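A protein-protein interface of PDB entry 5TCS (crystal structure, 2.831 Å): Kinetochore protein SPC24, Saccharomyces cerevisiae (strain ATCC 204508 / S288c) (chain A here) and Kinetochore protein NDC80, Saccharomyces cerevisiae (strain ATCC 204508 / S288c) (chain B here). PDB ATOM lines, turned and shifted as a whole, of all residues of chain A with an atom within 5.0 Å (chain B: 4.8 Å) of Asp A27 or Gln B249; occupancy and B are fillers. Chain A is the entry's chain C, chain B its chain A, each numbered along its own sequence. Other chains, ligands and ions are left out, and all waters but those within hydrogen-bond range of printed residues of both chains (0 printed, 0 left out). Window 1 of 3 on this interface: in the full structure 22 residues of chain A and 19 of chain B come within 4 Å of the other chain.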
ATOM      1  N   ASP A  23      18.033  31.510  -3.379  1.00  0.00           N
ATOM      2  CA  ASP A  23      18.321  30.328  -2.572  1.00  0.00           C
ATOM      3  C   ASP A  23      19.817  30.242  -2.290  1.00  0.00           C
ATOM      4  O   ASP A  23      20.610  29.945  -3.188  1.00  0.00           O
ATOM      5  CB  ASP A  23      17.826  29.075  -3.287  1.00  0.00           C
ATOM      6  CG  ASP A  23      17.555  27.928  -2.332  1.00  0.00           C
ATOM      7  OD1 ASP A  23      18.201  27.877  -1.265  1.00  0.00           O
ATOM      8  OD2 ASP A  23      16.693  27.080  -2.647  1.00  0.00           O
ATOM      9  N   ILE A  24      20.200  30.494  -1.040  1.00  0.00           N
ATOM     10  CA  ILE A  24      21.609  30.455  -0.652  1.00  0.00           C
ATOM     11  C   ILE A  24      22.052  29.023  -0.375  1.00  0.00           C
ATOM     12  O   ILE A  24      23.031  28.527  -0.948  1.00  0.00           O
ATOM     13  CB  ILE A  24      21.846  31.360   0.573  1.00  0.00           C
ATOM     14  CG1 ILE A  24      21.659  32.830   0.180  1.00  0.00           C
ATOM     15  CG2 ILE A  24      23.233  31.107   1.183  1.00  0.00           C
ATOM     16  CD1 ILE A  24      21.960  33.830   1.289  1.00  0.00           C
ATOM     17  N   GLN A  25      21.338  28.343   0.526  1.00  0.00           N
ATOM     18  CA  GLN A  25      21.752  27.011   0.949  1.00  0.00           C
ATOM     19  C   GLN A  25      21.832  26.052  -0.229  1.00  0.00           C
ATOM     20  O   GLN A  25      22.575  25.067  -0.175  1.00  0.00           O
ATOM     21  CB  GLN A  25      20.786  26.473   2.004  1.00  0.00           C
ATOM     22  CG  GLN A  25      21.349  25.318   2.815  1.00  0.00           C
ATOM     23  CD  GLN A  25      22.507  25.743   3.700  1.00  0.00           C
ATOM     24  OE1 GLN A  25      22.395  26.698   4.470  1.00  0.00           O
ATOM     25  NE2 GLN A  25      23.630  25.042   3.587  1.00  0.00           N
ATOM     26  N   GLN A  26      21.077  26.314  -1.295  1.00  0.00           N
ATOM     27  CA  GLN A  26      21.143  25.458  -2.473  1.00  0.00           C
ATOM     28  C   GLN A  26      22.524  25.524  -3.115  1.00  0.00           C
ATOM     29  O   GLN A  26      23.170  24.492  -3.339  1.00  0.00           O
ATOM     30  CB  GLN A  26      20.060  25.866  -3.470  1.00  0.00           C
ATOM     31  CG  GLN A  26      20.009  25.006  -4.718  1.00  0.00           C
ATOM     32  CD  GLN A  26      18.814  25.331  -5.590  1.00  0.00           C
ATOM     33  OE1 GLN A  26      17.670  25.078  -5.212  1.00  0.00           O
ATOM     34  NE2 GLN A  26      19.073  25.903  -6.760  1.00  0.00           N
ATOM     35  N   ASP A  27      22.999  26.736  -3.407  1.00  0.00           N
ATOM     36  CA  ASP A  27      24.313  26.884  -4.023  1.00  0.00           C
ATOM     37  C   ASP A  27      25.423  26.476  -3.065  1.00  0.00           C
ATOM     38  O   ASP A  27      26.433  25.903  -3.491  1.00  0.00           O
ATOM     39  CB  ASP A  27      24.514  28.322  -4.494  1.00  0.00           C
ATOM     40  CG  ASP A  27      23.656  28.664  -5.691  1.00  0.00           C
ATOM     41  OD1 ASP A  27      23.002  27.752  -6.240  1.00  0.00           O
ATOM     42  OD2 ASP A  27      23.640  29.845  -6.088  1.00  0.00           O
ATOM     43  N   VAL A  28      25.271  26.770  -1.773  1.00  0.00           N
ATOM     44  CA  VAL A  28      26.257  26.304  -0.801  1.00  0.00           C
ATOM     45  C   VAL A  28      26.368  24.784  -0.858  1.00  0.00           C
ATOM     46  O   VAL A  28      27.465  24.224  -0.997  1.00  0.00           O
ATOM     47  CB  VAL A  28      25.894  26.797   0.612  1.00  0.00           C
ATOM     48  CG1 VAL A  28      26.665  26.023   1.679  1.00  0.00           C
ATOM     49  CG2 VAL A  28      26.183  28.281   0.734  1.00  0.00           C
ATOM     50  N   ASP A  29      25.230  24.095  -0.754  1.00  0.00           N
ATOM     51  CA  ASP A  29      25.228  22.641  -0.871  1.00  0.00           C
ATOM     52  C   ASP A  29      25.888  22.197  -2.168  1.00  0.00           C
ATOM     53  O   ASP A  29      26.625  21.204  -2.193  1.00  0.00           O
ATOM     54  CB  ASP A  29      23.795  22.113  -0.789  1.00  0.00           C
ATOM     55  CG  ASP A  29      23.240  22.148   0.624  1.00  0.00           C
ATOM     56  OD1 ASP A  29      23.850  22.812   1.487  1.00  0.00           O
ATOM     57  OD2 ASP A  29      22.191  21.514   0.871  1.00  0.00           O
ATOM     58  N   ALA A  30      25.636  22.921  -3.261  1.00  0.00           N
ATOM     59  CA  ALA A  30      26.300  22.601  -4.520  1.00  0.00           C
ATOM     60  C   ALA A  30      27.816  22.680  -4.375  1.00  0.00           C
ATOM     61  O   ALA A  30      28.537  21.804  -4.864  1.00  0.00           O
ATOM     62  CB  ALA A  30      25.815  23.540  -5.624  1.00  0.00           C
ATOM     63  N   MET A  31      28.317  23.715  -3.708  1.00  0.00           N
ATOM     64  CA  MET A  31      29.756  23.857  -3.512  1.00  0.00           C
ATOM     65  C   MET A  31      30.295  22.684  -2.706  1.00  0.00           C
ATOM     66  O   MET A  31      31.379  22.175  -2.989  1.00  0.00           O
ATOM     67  CB  MET A  31      30.095  25.173  -2.804  1.00  0.00           C
ATOM     68  CG  MET A  31      30.117  26.408  -3.698  1.00  0.00           C
ATOM     69  SD  MET A  31      31.391  26.355  -5.186  1.00  0.00           S
ATOM     70  CE  MET A  31      32.679  25.035  -4.530  1.00  0.00           C
ATOM     71  N   LYS B 245      22.448  35.719 -10.170  1.00  0.00           N
ATOM     72  CA  LYS B 245      22.114  34.397  -9.653  1.00  0.00           C
ATOM     73  C   LYS B 245      22.208  33.359 -10.764  1.00  0.00           C
ATOM     74  O   LYS B 245      22.982  32.401 -10.677  1.00  0.00           O
ATOM     75  CB  LYS B 245      20.712  34.426  -9.042  1.00  0.00           C
ATOM     76  CG  LYS B 245      20.251  33.110  -8.449  1.00  0.00           C
ATOM     77  CD  LYS B 245      21.168  32.645  -7.330  1.00  0.00           C
ATOM     78  CE  LYS B 245      20.557  31.473  -6.586  1.00  0.00           C
ATOM     79  NZ  LYS B 245      21.542  30.822  -5.696  1.00  0.00           N
ATOM     80  N   ILE B 246      21.458  33.571 -11.846  1.00  0.00           N
ATOM     81  CA  ILE B 246      21.414  32.666 -12.993  1.00  0.00           C
ATOM     82  C   ILE B 246      22.855  32.300 -13.323  1.00  0.00           C
ATOM     83  O   ILE B 246      23.233  31.122 -13.270  1.00  0.00           O
ATOM     84  CB  ILE B 246      20.686  33.303 -14.200  1.00  0.00           C
ATOM     85  CG1 ILE B 246      19.178  33.046 -14.106  1.00  0.00           C
ATOM     86  CG2 ILE B 246      21.212  32.743 -15.526  1.00  0.00           C
ATOM     87  CD1 ILE B 246      18.552  33.407 -12.766  1.00  0.00           C
ATOM     88  N   ASN B 247      23.669  33.312 -13.620  1.00  0.00           N
ATOM     89  CA  ASN B 247      25.034  33.044 -14.048  1.00  0.00           C
ATOM     90  C   ASN B 247      25.727  32.111 -13.065  1.00  0.00           C
ATOM     91  O   ASN B 247      26.237  31.052 -13.450  1.00  0.00           O
ATOM     92  CB  ASN B 247      25.812  34.352 -14.202  1.00  0.00           C
ATOM     93  CG  ASN B 247      27.159  34.154 -14.876  1.00  0.00           C
ATOM     94  OD1 ASN B 247      28.193  34.557 -14.347  1.00  0.00           O
ATOM     95  ND2 ASN B 247      27.153  33.515 -16.043  1.00  0.00           N
ATOM     96  N   ILE B 248      25.720  32.467 -11.776  1.00  0.00           N
ATOM     97  CA  ILE B 248      26.393  31.637 -10.781  1.00  0.00           C
ATOM     98  C   ILE B 248      25.904  30.201 -10.895  1.00  0.00           C
ATOM     99  O   ILE B 248      26.697  29.258 -10.998  1.00  0.00           O
ATOM    100  CB  ILE B 248      26.166  32.184  -9.360  1.00  0.00           C
ATOM    101  CG1 ILE B 248      26.603  33.651  -9.245  1.00  0.00           C
ATOM    102  CG2 ILE B 248      26.912  31.316  -8.350  1.00  0.00           C
ATOM    103  CD1 ILE B 248      28.101  33.873  -9.314  1.00  0.00           C
ATOM    104  N   GLN B 249      24.582  30.020 -10.898  1.00  0.00           N
ATOM    105  CA  GLN B 249      24.034  28.672 -10.958  1.00  0.00           C
ATOM    106  C   GLN B 249      24.574  27.930 -12.172  1.00  0.00           C
ATOM    107  O   GLN B 249      24.998  26.773 -12.063  1.00  0.00           O
ATOM    108  CB  GLN B 249      22.505  28.725 -10.975  1.00  0.00           C
ATOM    109  CG  GLN B 249      21.918  29.539  -9.826  1.00  0.00           C
ATOM    110  CD  GLN B 249      20.744  28.859  -9.148  1.00  0.00           C
ATOM    111  OE1 GLN B 249      20.809  28.513  -7.967  1.00  0.00           O
ATOM    112  NE2 GLN B 249      19.656  28.675  -9.888  1.00  0.00           N
ATOM    113  N   SER B 250      24.608  28.595 -13.329  1.00  0.00           N
ATOM    114  CA  SER B 250      25.207  27.988 -14.510  1.00  0.00           C
ATOM    115  C   SER B 250      26.602  27.471 -14.186  1.00  0.00           C
ATOM    116  O   SER B 250      26.894  26.280 -14.346  1.00  0.00           O
ATOM    117  CB  SER B 250      25.248  29.004 -15.654  1.00  0.00           C
ATOM    118  OG  SER B 250      25.858  28.447 -16.807  1.00  0.00           O
ATOM    119  N   SER B 251      27.468  28.359 -13.685  1.00  0.00           N
ATOM    120  CA  SER B 251      28.828  27.962 -13.341  1.00  0.00           C
ATOM    121  C   SER B 251      28.837  26.704 -12.485  1.00  0.00           C
ATOM    122  O   SER B 251      29.687  25.824 -12.667  1.00  0.00           O
ATOM    123  CB  SER B 251      29.540  29.105 -12.615  1.00  0.00           C
ATOM    124  OG  SER B 251      29.881  30.146 -13.512  1.00  0.00           O
ATOM    125  N   LEU B 252      27.893  26.597 -11.549  1.00  0.00           N
ATOM    126  CA  LEU B 252      27.827  25.406 -10.710  1.00  0.00           C
ATOM    127  C   LEU B 252      27.377  24.200 -11.521  1.00  0.00           C
ATOM    128  O   LEU B 252      28.048  23.159 -11.533  1.00  0.00           O
ATOM    129  CB  LEU B 252      26.884  25.646  -9.531  1.00  0.00           C
ATOM    130  CG  LEU B 252      27.294  26.738  -8.538  1.00  0.00           C
ATOM    131  CD1 LEU B 252      26.163  27.025  -7.567  1.00  0.00           C
ATOM    132  CD2 LEU B 252      28.552  26.343  -7.780  1.00  0.00           C
ATOM    133  N   GLU B 253      26.255  24.331 -12.233  1.00  0.00           N
ATOM    134  CA  GLU B 253      25.681  23.186 -12.932  1.00  0.00           C
ATOM    135  C   GLU B 253      26.703  22.552 -13.866  1.00  0.00           C
ATOM    136  O   GLU B 253      26.847  21.324 -13.908  1.00  0.00           O
ATOM    137  CB  GLU B 253      24.438  23.618 -13.706  1.00  0.00           C
ATOM    138  CG  GLU B 253      23.600  22.461 -14.207  1.00  0.00           C
ATOM    139  CD  GLU B 253      22.318  22.916 -14.874  1.00  0.00           C
ATOM    140  OE1 GLU B 253      22.338  23.965 -15.554  1.00  0.00           O
ATOM    141  OE2 GLU B 253      21.287  22.228 -14.714  1.00  0.00           O
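NE2 of Gln A26 sits at hydrogen-bond distance from OE1 of Gln B249 (3.4 Å). NZ of Lys B245 lies within salt-bridge range of OD1 of Asp A27. NZ of Lys B245 lies within hydrogen-bond range of O of Asp A23. OD1 of Asp A27 sits close to OE1 of Gln B249 (2.9 Å).
The side-chain amino group of Lys B245 sits close to the side-chain amide oxygen of Gln B249, 3.3 Å away. OD1 of Asp A23 is in hydrogen-bond range of N of Gln A26, at 3.3 Å.
Among the printed residues, merely in contact across the chains: Asp A27 with Leu B252 (3.5 Å) and Met A31 with Leu B252 (3.8 Å).
Gln B249 touches just these residues of chain A: Gln A26 (3.4 Å) and Asp A27 (2.9 Å). Printed residues of chain B within 4 Å of Gln A26: Gln B249. Of the printed residues of chain B, Met A31 touches Leu B252 (3.8 Å). Of the printed residues of chain A, Lys B245 touches Asp A23 and Asp A27. Of the printed residues of chain A, Leu B252 touches Asp A27 and Met A31. Of the printed residues of chain B, Asp A23 touches Lys B245 (2.8 Å). Ile B248 touches none of the printed residues of chain A. The nearest residue of chain B that does not touch Asp A27 is Ile B248 (4.2 Å). The nearest printed residue of chain A that does not touch Lys B245 is Ile A24 (4.9 Å).
Of the 9 printed residues of chain B, 3 touch a printed residue of chain A. Of the 9 printed residues of chain A, 4 touch a printed residue of chain B. Hydrophobic or aromatic side chains of chain A that line the printed part of chain B: Met A31. Along chain A the printed residues that touch a printed residue of chain B span positions 23 to 31. Among the printed residues, Asp or Glu carboxylates within 4 Å of a Lys or Arg side-chain nitrogen of the other chain: Asp A27 with Lys B245.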
